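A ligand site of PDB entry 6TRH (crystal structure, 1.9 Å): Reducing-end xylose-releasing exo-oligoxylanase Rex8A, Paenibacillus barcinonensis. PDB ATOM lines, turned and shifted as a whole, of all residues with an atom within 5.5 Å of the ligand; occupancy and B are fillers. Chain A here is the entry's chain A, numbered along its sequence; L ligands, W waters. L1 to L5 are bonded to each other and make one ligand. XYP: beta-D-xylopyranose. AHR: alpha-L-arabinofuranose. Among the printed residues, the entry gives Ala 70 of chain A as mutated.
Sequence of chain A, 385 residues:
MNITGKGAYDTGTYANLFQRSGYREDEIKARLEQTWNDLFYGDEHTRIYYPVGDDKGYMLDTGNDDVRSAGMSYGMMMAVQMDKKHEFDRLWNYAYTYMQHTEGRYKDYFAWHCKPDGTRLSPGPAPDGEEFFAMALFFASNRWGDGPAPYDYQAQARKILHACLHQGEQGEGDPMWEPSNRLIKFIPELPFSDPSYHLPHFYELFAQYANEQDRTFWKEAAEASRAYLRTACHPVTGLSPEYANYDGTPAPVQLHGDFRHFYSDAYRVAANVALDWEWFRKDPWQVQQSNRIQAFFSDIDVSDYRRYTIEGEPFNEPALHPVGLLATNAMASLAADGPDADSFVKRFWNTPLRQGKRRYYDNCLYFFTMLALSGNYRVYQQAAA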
ATOM      1  N   ASP A  61      23.583  -5.713 -15.908  1.00  0.00           N
ATOM      2  CA  ASP A  61      25.056  -5.947 -15.935  1.00  0.00           C
ATOM      3  C   ASP A  61      25.463  -6.430 -14.544  1.00  0.00           C
ATOM      4  O   ASP A  61      25.815  -5.578 -13.690  1.00  0.00           O
ATOM      5  CB  ASP A  61      25.833  -4.712 -16.387  1.00  0.00           C
ATOM      6  CG  ASP A  61      27.328  -4.954 -16.554  1.00  0.00           C
ATOM      7  OD1 ASP A  61      27.858  -5.869 -15.878  1.00  0.00           O
ATOM      8  OD2 ASP A  61      27.957  -4.229 -17.349  1.00  0.00           O
ATOM      9  N   ASN A  64      28.727  -5.227 -13.022  1.00  0.00           N
ATOM     10  CA  ASN A  64      28.823  -3.802 -12.580  1.00  0.00           C
ATOM     11  C   ASN A  64      27.604  -3.397 -11.736  1.00  0.00           C
ATOM     12  O   ASN A  64      27.577  -2.241 -11.301  1.00  0.00           O
ATOM     13  CB  ASN A  64      29.044  -2.895 -13.779  1.00  0.00           C
ATOM     14  CG  ASN A  64      30.421  -3.059 -14.383  1.00  0.00           C
ATOM     15  OD1 ASN A  64      31.430  -2.895 -13.697  1.00  0.00           O
ATOM     16  ND2 ASN A  64      30.483  -3.384 -15.670  1.00  0.00           N
ATOM     17  N   ARG A  68      22.512  -1.065 -18.256  1.00  0.00           N
ATOM     18  CA  ARG A  68      23.181  -0.308 -19.347  1.00  0.00           C
ATOM     19  C   ARG A  68      22.223  -0.165 -20.540  1.00  0.00           C
ATOM     20  O   ARG A  68      21.279  -0.972 -20.629  1.00  0.00           O
ATOM     21  CB  ARG A  68      24.493  -0.980 -19.775  1.00  0.00           C
ATOM     22  CG  ARG A  68      25.708  -0.505 -18.989  1.00  0.00           C
ATOM     23  CD  ARG A  68      26.619  -1.632 -18.548  1.00  0.00           C
ATOM     24  NE  ARG A  68      27.414  -1.246 -17.383  1.00  0.00           N
ATOM     25  CZ  ARG A  68      28.707  -0.920 -17.370  1.00  0.00           C
ATOM     26  NH1 ARG A  68      29.443  -0.957 -18.473  1.00  0.00           N
ATOM     27  NH2 ARG A  68      29.276  -0.573 -16.232  1.00  0.00           N
ATOM     28  N   SER A  69      22.460   0.836 -21.398  1.00  0.00           N
ATOM     29  CA  SER A  69      21.651   1.119 -22.611  1.00  0.00           C
ATOM     30  C   SER A  69      21.911   0.011 -23.644  1.00  0.00           C
ATOM     31  O   SER A  69      20.937  -0.506 -24.225  1.00  0.00           O
ATOM     32  CB  SER A  69      21.932   2.501 -23.168  1.00  0.00           C
ATOM     33  OG  SER A  69      23.208   2.590 -23.773  1.00  0.00           O
ATOM     34  N   ALA A  70      23.181  -0.363 -23.819  1.00  0.00           N
ATOM     35  CA  ALA A  70      23.662  -1.470 -24.681  1.00  0.00           C
ATOM     36  C   ALA A  70      22.938  -2.774 -24.315  1.00  0.00           C
ATOM     37  O   ALA A  70      22.481  -3.497 -25.238  1.00  0.00           O
ATOM     38  CB  ALA A  70      25.149  -1.619 -24.536  1.00  0.00           C
ATOM     39  N   TYR A  74      20.206  -4.806 -26.427  1.00  0.00           N
ATOM     40  CA  TYR A  74      20.501  -6.243 -26.703  1.00  0.00           C
ATOM     41  C   TYR A  74      19.258  -7.078 -26.354  1.00  0.00           C
ATOM     42  O   TYR A  74      18.895  -7.965 -27.163  1.00  0.00           O
ATOM     43  CB  TYR A  74      21.682  -6.777 -25.882  1.00  0.00           C
ATOM     44  CG  TYR A  74      23.054  -6.303 -26.269  1.00  0.00           C
ATOM     45  CD1 TYR A  74      23.312  -5.658 -27.474  1.00  0.00           C
ATOM     46  CD2 TYR A  74      24.121  -6.548 -25.423  1.00  0.00           C
ATOM     47  CE1 TYR A  74      24.591  -5.235 -27.792  1.00  0.00           C
ATOM     48  CE2 TYR A  74      25.406  -6.152 -25.738  1.00  0.00           C
ATOM     49  CZ  TYR A  74      25.640  -5.489 -26.923  1.00  0.00           C
ATOM     50  OH  TYR A  74      26.907  -5.103 -27.217  1.00  0.00           O
ATOM     51  N   TRP A 112      23.302   6.298 -20.427  1.00  0.00           N
ATOM     52  CA  TRP A 112      24.008   5.057 -20.861  1.00  0.00           C
ATOM     53  C   TRP A 112      23.930   3.960 -19.779  1.00  0.00           C
ATOM     54  O   TRP A 112      24.001   2.782 -20.163  1.00  0.00           O
ATOM     55  CB  TRP A 112      25.453   5.344 -21.323  1.00  0.00           C
ATOM     56  CG  TRP A 112      26.491   5.492 -20.254  1.00  0.00           C
ATOM     57  CD1 TRP A 112      26.963   6.655 -19.720  1.00  0.00           C
ATOM     58  CD2 TRP A 112      27.257   4.443 -19.644  1.00  0.00           C
ATOM     59  NE1 TRP A 112      27.950   6.400 -18.798  1.00  0.00           N
ATOM     60  CE2 TRP A 112      28.147   5.045 -18.737  1.00  0.00           C
ATOM     61  CE3 TRP A 112      27.277   3.044 -19.772  1.00  0.00           C
ATOM     62  CZ2 TRP A 112      29.045   4.304 -17.953  1.00  0.00           C
ATOM     63  CZ3 TRP A 112      28.149   2.317 -19.009  1.00  0.00           C
ATOM     64  CH2 TRP A 112      29.021   2.929 -18.112  1.00  0.00           C
ATOM     65  N   HIS A 113      23.789   4.310 -18.501  1.00  0.00           N
ATOM     66  CA  HIS A 113      23.540   3.336 -17.404  1.00  0.00           C
ATOM     67  C   HIS A 113      22.802   3.992 -16.224  1.00  0.00           C
ATOM     68  O   HIS A 113      23.013   5.199 -15.985  1.00  0.00           O
ATOM     69  CB  HIS A 113      24.840   2.640 -16.974  1.00  0.00           C
ATOM     70  CG  HIS A 113      25.719   3.449 -16.077  1.00  0.00           C
ATOM     71  ND1 HIS A 113      26.324   4.618 -16.505  1.00  0.00           N
ATOM     72  CD2 HIS A 113      26.115   3.244 -14.805  1.00  0.00           C
ATOM     73  CE1 HIS A 113      27.056   5.104 -15.519  1.00  0.00           C
ATOM     74  NE2 HIS A 113      26.942   4.287 -14.474  1.00  0.00           N
ATOM     75  N   SER A 122      24.879   8.089 -14.881  1.00  0.00           N
ATOM     76  CA  SER A 122      25.455   9.120 -15.786  1.00  0.00           C
ATOM     77  C   SER A 122      24.382   9.575 -16.775  1.00  0.00           C
ATOM     78  O   SER A 122      23.563   8.765 -17.201  1.00  0.00           O
ATOM     79  CB  SER A 122      26.674   8.588 -16.506  1.00  0.00           C
ATOM     80  OG  SER A 122      27.652   8.149 -15.576  1.00  0.00           O
ATOM     81  N   PRO A 123      24.324  10.875 -17.138  1.00  0.00           N
ATOM     82  CA  PRO A 123      23.346  11.370 -18.105  1.00  0.00           C
ATOM     83  C   PRO A 123      23.746  11.106 -19.563  1.00  0.00           C
ATOM     84  O   PRO A 123      22.866  10.879 -20.379  1.00  0.00           O
ATOM     85  CB  PRO A 123      23.306  12.874 -17.806  1.00  0.00           C
ATOM     86  CG  PRO A 123      24.723  13.189 -17.363  1.00  0.00           C
ATOM     87  CD  PRO A 123      25.192  11.954 -16.611  1.00  0.00           C
ATOM     88  N   GLY A 124      25.048  11.136 -19.861  1.00  0.00           N
ATOM     89  CA  GLY A 124      25.616  10.935 -21.213  1.00  0.00           C
ATOM     90  C   GLY A 124      25.209   9.591 -21.812  1.00  0.00           C
ATOM     91  O   GLY A 124      24.875   8.656 -21.098  1.00  0.00           O
ATOM     92  N   PRO A 125      25.133   9.477 -23.155  1.00  0.00           N
ATOM     93  CA  PRO A 125      24.695   8.250 -23.825  1.00  0.00           C
ATOM     94  C   PRO A 125      25.778   7.356 -24.432  1.00  0.00           C
ATOM     95  O   PRO A 125      26.858   7.824 -24.635  1.00  0.00           O
ATOM     96  CB  PRO A 125      23.852   8.839 -24.968  1.00  0.00           C
ATOM     97  CG  PRO A 125      24.635  10.067 -25.358  1.00  0.00           C
ATOM     98  CD  PRO A 125      25.121  10.643 -24.050  1.00  0.00           C
ATOM     99  N   ALA A 126      25.433   6.102 -24.761  1.00  0.00           N
ATOM    100  CA  ALA A 126      26.317   5.152 -25.474  1.00  0.00           C
ATOM    101  C   ALA A 126      25.682   4.807 -26.831  1.00  0.00           C
ATOM    102  O   ALA A 126      24.632   4.171 -26.863  1.00  0.00           O
ATOM    103  CB  ALA A 126      26.551   3.923 -24.633  1.00  0.00           C
ATOM    104  N   ASP A 128      26.037   2.669 -29.291  1.00  0.00           N
ATOM    105  CA  ASP A 128      25.765   1.250 -29.627  1.00  0.00           C
ATOM    106  C   ASP A 128      24.392   0.854 -29.096  1.00  0.00           C
ATOM    107  O   ASP A 128      23.759  -0.004 -29.716  1.00  0.00           O
ATOM    108  CB  ASP A 128      26.894   0.320 -29.165  1.00  0.00           C
ATOM    109  CG  ASP A 128      27.213   0.395 -27.676  1.00  0.00           C
ATOM    110  OD1 ASP A 128      27.160   1.514 -27.106  1.00  0.00           O
ATOM    111  OD2 ASP A 128      27.536  -0.666 -27.117  1.00  0.00           O
ATOM    112  N   GLY A 129      23.923   1.483 -28.005  1.00  0.00           N
ATOM    113  CA  GLY A 129      22.568   1.303 -27.467  1.00  0.00           C
ATOM    114  C   GLY A 129      21.514   1.847 -28.425  1.00  0.00           C
ATOM    115  O   GLY A 129      20.630   1.066 -28.842  1.00  0.00           O
ATOM    116  N   PHE A 186      32.329   7.238 -30.637  1.00  0.00           N
ATOM    117  CA  PHE A 186      32.404   6.602 -29.297  1.00  0.00           C
ATOM    118  C   PHE A 186      31.332   7.242 -28.403  1.00  0.00           C
ATOM    119  O   PHE A 186      30.510   6.503 -27.830  1.00  0.00           O
ATOM    120  CB  PHE A 186      33.792   6.707 -28.681  1.00  0.00           C
ATOM    121  CG  PHE A 186      33.830   6.410 -27.203  1.00  0.00           C
ATOM    122  CD1 PHE A 186      33.217   5.269 -26.698  1.00  0.00           C
ATOM    123  CD2 PHE A 186      34.461   7.258 -26.310  1.00  0.00           C
ATOM    124  CE1 PHE A 186      33.235   4.992 -25.342  1.00  0.00           C
ATOM    125  CE2 PHE A 186      34.480   6.981 -24.955  1.00  0.00           C
ATOM    126  CZ  PHE A 186      33.862   5.851 -24.470  1.00  0.00           C
ATOM    127  N   ILE A 187      31.358   8.563 -28.279  1.00  0.00           N
ATOM    128  CA  ILE A 187      30.279   9.388 -27.645  1.00  0.00           C
ATOM    129  C   ILE A 187      30.131  10.661 -28.465  1.00  0.00           C
ATOM    130  O   ILE A 187      30.994  10.986 -29.279  1.00  0.00           O
ATOM    131  CB  ILE A 187      30.587   9.671 -26.158  1.00  0.00           C
ATOM    132  CG1 ILE A 187      31.895  10.439 -25.969  1.00  0.00           C
ATOM    133  CG2 ILE A 187      30.572   8.382 -25.340  1.00  0.00           C
ATOM    134  CD1 ILE A 187      32.029  11.134 -24.638  1.00  0.00           C
ATOM    135  N   LEU A 190      33.471  13.301 -28.342  1.00  0.00           N
ATOM    136  CA  LEU A 190      34.877  12.950 -28.686  1.00  0.00           C
ATOM    137  C   LEU A 190      34.984  12.595 -30.163  1.00  0.00           C
ATOM    138  O   LEU A 190      34.146  11.846 -30.675  1.00  0.00           O
ATOM    139  CB  LEU A 190      35.337  11.800 -27.781  1.00  0.00           C
ATOM    140  CG  LEU A 190      35.504  12.158 -26.306  1.00  0.00           C
ATOM    141  CD1 LEU A 190      35.570  10.907 -25.445  1.00  0.00           C
ATOM    142  CD2 LEU A 190      36.736  13.015 -26.083  1.00  0.00           C
ATOM    143  N   TYR A 197      31.096  -0.812 -32.542  1.00  0.00           N
ATOM    144  CA  TYR A 197      29.855  -0.010 -32.684  1.00  0.00           C
ATOM    145  C   TYR A 197      29.367  -0.032 -34.141  1.00  0.00           C
ATOM    146  O   TYR A 197      28.199   0.319 -34.380  1.00  0.00           O
ATOM    147  CB  TYR A 197      30.061   1.422 -32.207  1.00  0.00           C
ATOM    148  CG  TYR A 197      30.172   1.618 -30.702  1.00  0.00           C
ATOM    149  CD1 TYR A 197      30.469   0.564 -29.851  1.00  0.00           C
ATOM    150  CD2 TYR A 197      30.043   2.879 -30.143  1.00  0.00           C
ATOM    151  CE1 TYR A 197      30.602   0.751 -28.487  1.00  0.00           C
ATOM    152  CE2 TYR A 197      30.160   3.077 -28.780  1.00  0.00           C
ATOM    153  CZ  TYR A 197      30.451   2.014 -27.937  1.00  0.00           C
ATOM    154  OH  TYR A 197      30.572   2.182 -26.591  1.00  0.00           O
ATOM    155  N   TYR A 243      38.863   1.026 -28.546  1.00  0.00           N
ATOM    156  CA  TYR A 243      38.653   2.399 -29.081  1.00  0.00           C
ATOM    157  C   TYR A 243      39.642   2.649 -30.225  1.00  0.00           C
ATOM    158  O   TYR A 243      40.836   2.317 -30.079  1.00  0.00           O
ATOM    159  CB  TYR A 243      38.846   3.476 -28.003  1.00  0.00           C
ATOM    160  CG  TYR A 243      37.921   3.442 -26.814  1.00  0.00           C
ATOM    161  CD1 TYR A 243      36.768   2.665 -26.777  1.00  0.00           C
ATOM    162  CD2 TYR A 243      38.193   4.234 -25.710  1.00  0.00           C
ATOM    163  CE1 TYR A 243      35.948   2.661 -25.666  1.00  0.00           C
ATOM    164  CE2 TYR A 243      37.370   4.246 -24.591  1.00  0.00           C
ATOM    165  CZ  TYR A 243      36.241   3.450 -24.572  1.00  0.00           C
ATOM    166  OH  TYR A 243      35.431   3.461 -23.484  1.00  0.00           O
ATOM    167  N   HIS A 256      39.744   6.848 -18.166  1.00  0.00           N
ATOM    168  CA  HIS A 256      38.953   5.766 -17.518  1.00  0.00           C
ATOM    169  C   HIS A 256      39.497   4.382 -17.911  1.00  0.00           C
ATOM    170  O   HIS A 256      38.923   3.377 -17.442  1.00  0.00           O
ATOM    171  CB  HIS A 256      37.453   5.926 -17.825  1.00  0.00           C
ATOM    172  CG  HIS A 256      37.119   5.867 -19.274  1.00  0.00           C
ATOM    173  ND1 HIS A 256      37.240   6.966 -20.117  1.00  0.00           N
ATOM    174  CD2 HIS A 256      36.677   4.855 -20.047  1.00  0.00           C
ATOM    175  CE1 HIS A 256      36.889   6.626 -21.335  1.00  0.00           C
ATOM    176  NE2 HIS A 256      36.533   5.329 -21.327  1.00  0.00           N
ATOM    177  N   SER A 264      37.218  -6.714 -24.268  1.00  0.00           N
ATOM    178  CA  SER A 264      35.758  -7.023 -24.236  1.00  0.00           C
ATOM    179  C   SER A 264      35.011  -6.434 -25.453  1.00  0.00           C
ATOM    180  O   SER A 264      34.299  -7.215 -26.138  1.00  0.00           O
ATOM    181  CB  SER A 264      35.133  -6.522 -22.964  1.00  0.00           C
ATOM    182  OG  SER A 264      35.891  -6.927 -21.826  1.00  0.00           O
ATOM    183  N   ASP A 265      35.119  -5.127 -25.683  1.00  0.00           N
ATOM    184  CA  ASP A 265      34.351  -4.396 -26.733  1.00  0.00           C
ATOM    185  C   ASP A 265      34.646  -5.011 -28.110  1.00  0.00           C
ATOM    186  O   ASP A 265      33.683  -5.328 -28.833  1.00  0.00           O
ATOM    187  CB  ASP A 265      34.648  -2.894 -26.739  1.00  0.00           C
ATOM    188  CG  ASP A 265      33.872  -2.079 -25.715  1.00  0.00           C
ATOM    189  OD1 ASP A 265      33.603  -2.615 -24.632  1.00  0.00           O
ATOM    190  OD2 ASP A 265      33.544  -0.923 -26.022  1.00  0.00           O
ATOM    191  N   ARG A 268      32.988  -8.181 -30.451  1.00  0.00           N
ATOM    192  CA  ARG A 268      31.718  -8.086 -31.233  1.00  0.00           C
ATOM    193  C   ARG A 268      32.014  -7.785 -32.706  1.00  0.00           C
ATOM    194  O   ARG A 268      31.111  -8.010 -33.520  1.00  0.00           O
ATOM    195  CB  ARG A 268      30.797  -7.030 -30.620  1.00  0.00           C
ATOM    196  CG  ARG A 268      30.245  -7.385 -29.253  1.00  0.00           C
ATOM    197  CD  ARG A 268      29.552  -6.245 -28.527  1.00  0.00           C
ATOM    198  NE  ARG A 268      30.478  -5.157 -28.194  1.00  0.00           N
ATOM    199  CZ  ARG A 268      30.169  -4.081 -27.468  1.00  0.00           C
ATOM    200  NH1 ARG A 268      28.951  -3.914 -26.982  1.00  0.00           N
ATOM    201  NH2 ARG A 268      31.089  -3.158 -27.239  1.00  0.00           N
ATOM    202  N   LEU A 320      38.510 -11.016 -19.541  1.00  0.00           N
ATOM    203  CA  LEU A 320      37.439 -10.932 -18.519  1.00  0.00           C
ATOM    204  C   LEU A 320      36.230 -11.761 -18.977  1.00  0.00           C
ATOM    205  O   LEU A 320      35.519 -12.294 -18.108  1.00  0.00           O
ATOM    206  CB  LEU A 320      37.069  -9.465 -18.283  1.00  0.00           C
ATOM    207  CG  LEU A 320      35.949  -9.198 -17.288  1.00  0.00           C
ATOM    208  CD1 LEU A 320      36.187  -9.878 -15.950  1.00  0.00           C
ATOM    209  CD2 LEU A 320      35.743  -7.697 -17.092  1.00  0.00           C
ATOM    210  N   HIS A 321      36.031 -11.901 -20.292  1.00  0.00           N
ATOM    211  CA  HIS A 321      34.836 -12.545 -20.901  1.00  0.00           C
ATOM    212  C   HIS A 321      35.238 -13.578 -21.948  1.00  0.00           C
ATOM    213  O   HIS A 321      34.935 -13.408 -23.130  1.00  0.00           O
ATOM    214  CB  HIS A 321      33.898 -11.465 -21.467  1.00  0.00           C
ATOM    215  CG  HIS A 321      33.448 -10.453 -20.456  1.00  0.00           C
ATOM    216  ND1 HIS A 321      32.629 -10.774 -19.393  1.00  0.00           N
ATOM    217  CD2 HIS A 321      33.697  -9.134 -20.361  1.00  0.00           C
ATOM    218  CE1 HIS A 321      32.397  -9.690 -18.690  1.00  0.00           C
ATOM    219  NE2 HIS A 321      33.050  -8.676 -19.254  1.00  0.00           N
ATOM    220  N   TYR A 360      27.109 -11.618 -17.417  1.00  0.00           N
ATOM    221  CA  TYR A 360      26.182 -10.795 -18.258  1.00  0.00           C
ATOM    222  C   TYR A 360      26.719 -10.690 -19.690  1.00  0.00           C
ATOM    223  O   TYR A 360      26.029 -11.181 -20.607  1.00  0.00           O
ATOM    224  CB  TYR A 360      25.922  -9.437 -17.593  1.00  0.00           C
ATOM    225  CG  TYR A 360      25.595  -8.302 -18.521  1.00  0.00           C
ATOM    226  CD1 TYR A 360      24.294  -8.056 -18.936  1.00  0.00           C
ATOM    227  CD2 TYR A 360      26.597  -7.461 -18.982  1.00  0.00           C
ATOM    228  CE1 TYR A 360      23.992  -7.010 -19.786  1.00  0.00           C
ATOM    229  CE2 TYR A 360      26.306  -6.398 -19.834  1.00  0.00           C
ATOM    230  CZ  TYR A 360      25.003  -6.173 -20.236  1.00  0.00           C
ATOM    231  OH  TYR A 360      24.732  -5.134 -21.077  1.00  0.00           O
ATOM    232  N   TYR A 361      27.894 -10.090 -19.891  1.00  0.00           N
ATOM    233  CA  TYR A 361      28.436  -9.788 -21.253  1.00  0.00           C
ATOM    234  C   TYR A 361      28.680 -11.080 -22.035  1.00  0.00           C
ATOM    235  O   TYR A 361      28.397 -11.106 -23.258  1.00  0.00           O
ATOM    236  CB  TYR A 361      29.715  -8.955 -21.160  1.00  0.00           C
ATOM    237  CG  TYR A 361      30.198  -8.407 -22.474  1.00  0.00           C
ATOM    238  CD1 TYR A 361      29.438  -7.481 -23.182  1.00  0.00           C
ATOM    239  CD2 TYR A 361      31.419  -8.797 -23.018  1.00  0.00           C
ATOM    240  CE1 TYR A 361      29.868  -6.956 -24.381  1.00  0.00           C
ATOM    241  CE2 TYR A 361      31.863  -8.269 -24.218  1.00  0.00           C
ATOM    242  CZ  TYR A 361      31.079  -7.362 -24.903  1.00  0.00           C
ATOM    243  OH  TYR A 361      31.505  -6.844 -26.091  1.00  0.00           O
HETATM  244  O1  XYP L   1      32.775  -5.924 -19.296  1.00  0.00           O
HETATM  245  C1  XYP L   1      31.837  -5.463 -20.321  1.00  0.00           C
HETATM  246  C2  XYP L   1      30.740  -4.683 -19.661  1.00  0.00           C
HETATM  247  C3  XYP L   1      29.828  -4.127 -20.748  1.00  0.00           C
HETATM  248  C4  XYP L   1      30.632  -3.338 -21.758  1.00  0.00           C
HETATM  249  C5  XYP L   1      31.524  -4.330 -22.397  1.00  0.00           C
HETATM  250  O2  XYP L   1      29.980  -5.557 -18.815  1.00  0.00           O
HETATM  251  O3  XYP L   1      28.900  -3.307 -20.150  1.00  0.00           O
HETATM  252  O4  XYP L   1      29.723  -2.714 -22.670  1.00  0.00           O
HETATM  253  O5  XYP L   1      32.465  -4.635 -21.338  1.00  0.00           O
HETATM  254  C1  XYP L   2      29.870  -1.245 -22.747  1.00  0.00           C
HETATM  255  C2  XYP L   2      28.923  -0.741 -23.756  1.00  0.00           C
HETATM  256  C3  XYP L   2      28.973   0.797 -23.867  1.00  0.00           C
HETATM  257  C4  XYP L   2      29.535   1.567 -22.621  1.00  0.00           C
HETATM  258  C5  XYP L   2      30.200   0.711 -21.564  1.00  0.00           C
HETATM  259  O2  XYP L   2      29.199  -1.347 -25.073  1.00  0.00           O
HETATM  260  O3  XYP L   2      27.611   1.218 -24.055  1.00  0.00           O
HETATM  261  O4  XYP L   2      30.489   2.540 -23.043  1.00  0.00           O
HETATM  262  O5  XYP L   2      29.557  -0.588 -21.504  1.00  0.00           O
HETATM  263  C1  XYP L   3      30.375   3.762 -22.158  1.00  0.00           C
HETATM  264  C2  XYP L   3      31.666   4.260 -21.478  1.00  0.00           C
HETATM  265  C3  XYP L   3      31.421   5.608 -20.722  1.00  0.00           C
HETATM  266  C4  XYP L   3      30.839   6.615 -21.768  1.00  0.00           C
HETATM  267  C5  XYP L   3      29.613   5.995 -22.438  1.00  0.00           C
HETATM  268  O2  XYP L   3      32.185   3.261 -20.582  1.00  0.00           O
HETATM  269  O3  XYP L   3      32.705   6.092 -20.080  1.00  0.00           O
HETATM  270  O4  XYP L   3      30.303   7.864 -21.271  1.00  0.00           O
HETATM  271  O5  XYP L   3      29.968   4.770 -23.081  1.00  0.00           O
HETATM  272  O5  AHR L   4      33.984   3.284 -16.020  1.00  0.00           O
HETATM  273  C5  AHR L   4      33.665   4.631 -15.633  1.00  0.00           C
HETATM  274  C4  AHR L   4      32.829   5.195 -16.743  1.00  0.00           C
HETATM  275  O4  AHR L   4      33.675   5.539 -17.860  1.00  0.00           O
HETATM  276  C3  AHR L   4      32.218   6.530 -16.322  1.00  0.00           C
HETATM  277  O3  AHR L   4      30.976   6.370 -15.540  1.00  0.00           O
HETATM  278  C2  AHR L   4      31.870   7.091 -17.644  1.00  0.00           C
HETATM  279  O2  AHR L   4      31.871   8.546 -17.442  1.00  0.00           O
HETATM  280  C1  AHR L   4      33.002   6.582 -18.614  1.00  0.00           C
HETATM  281  C1  XYP L   5      31.015   8.810 -20.693  1.00  0.00           C
HETATM  282  C2  XYP L   5      30.332   9.714 -19.712  1.00  0.00           C
HETATM  283  C3  XYP L   5      30.943  11.024 -20.124  1.00  0.00           C
HETATM  284  C4  XYP L   5      32.470  10.905 -20.386  1.00  0.00           C
HETATM  285  C5  XYP L   5      32.900   9.575 -21.012  1.00  0.00           C
HETATM  286  O2  XYP L   5      28.945   9.832 -19.888  1.00  0.00           O
HETATM  287  O3  XYP L   5      30.866  11.881 -19.032  1.00  0.00           O
HETATM  288  O4  XYP L   5      32.918  11.978 -21.220  1.00  0.00           O
HETATM  289  O5  XYP L   5      32.311   8.612 -20.294  1.00  0.00           O
HETATM  290  O   HOH W   1      35.581  -4.978 -20.244  1.00  0.00           O
HETATM  291  O   HOH W   2      33.752   1.631 -22.752  1.00  0.00           O
HETATM  292  O   HOH W   3      28.693  13.313 -21.455  1.00  0.00           O
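O2 of XYP L2 is in hydrogen-bond range of OD2 of Asp 128 (2.7 Å). A ring nitrogen (NE2) of His 321 lies within hydrogen-bond range of an oxygen (O1) of XYP L1. The side-chain carboxylate (OD2) of Asp 61 is in hydrogen-bond range of an oxygen (O2) of XYP L1, at 2.8 Å. O3 of XYP L1 lies within hydrogen-bond range of NH1 of Arg 68 (2.9 Å). NH1 of Arg 268 is in hydrogen-bond range of O2 of XYP L2, 3.2 Å away.
The side-chain carboxylate (OD2) of Asp 128 is in salt-bridge range of the guanidinium group (NH1) of Arg 268 (3.5 Å). ND2 of Asn 64 sits close to NH2 of Arg 68, at 3.1 Å. The guanidinium group (NH2) of Arg 268 is in salt-bridge range of the side-chain carboxylate (OD2) of Asp 265, at 3.5 Å. The guanidinium group (NE) of Arg 268 is in hydrogen-bond range of the side-chain hydroxyl (OH) of Tyr 361, at 2.9 Å. The backbone carbonyl oxygen of Gly 124 is in hydrogen-bond range of the backbone NH of Trp 112 (2.9 Å). A ring nitrogen (ND1) of His 113 sits close to the indole nitrogen (NE1) of Trp 112 (3.3 Å). The backbone NH (N) of Ser 69 lies within hydrogen-bond range of the backbone carbonyl oxygen (O) of Trp 112, 2.8 Å away. The side-chain hydroxyl of Tyr 243 sits at hydrogen-bond distance from a ring nitrogen (NE2) of His 256, 3.1 Å away.
Merely in contact with the ligand: Asn 64 (3.9 Å), Ala 70 (3.8 Å), Trp 112 (3.6 Å), Ser 122 (3.8 Å), Gly 124 (3.7 Å), Pro 125 (3.97 Å), Ala 126 (3.0 Å), Phe 186 (3.98 Å), Ile 187 (3.6 Å), Tyr 197 (3.4 Å), His 256 (3.7 Å), Ser 264 (3.7 Å), Asp 265 (3.5 Å), Tyr 360 (3.9 Å) and Tyr 361 (3.7 Å). Hydrophobic or aromatic side chains within 4 Å of the ligand: Ala 70, Trp 112, Ala 126, Phe 186, Ile 187, His 256, His 321, Tyr 360 and Tyr 361. Along chain A the residues within 4 Å of the ligand span positions 61 to 361.
Water W1 lies within hydrogen-bond range of the side-chain hydroxyl (OG) of Ser 264 (2.5 Å) and an oxygen (O1) of XYP L1 (3.1 Å). Water W2 lies within hydrogen-bond range of the side-chain hydroxyl (OH) of Tyr 243 (2.6 Å) and an oxygen (O2) of XYP L3 (3.1 Å).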
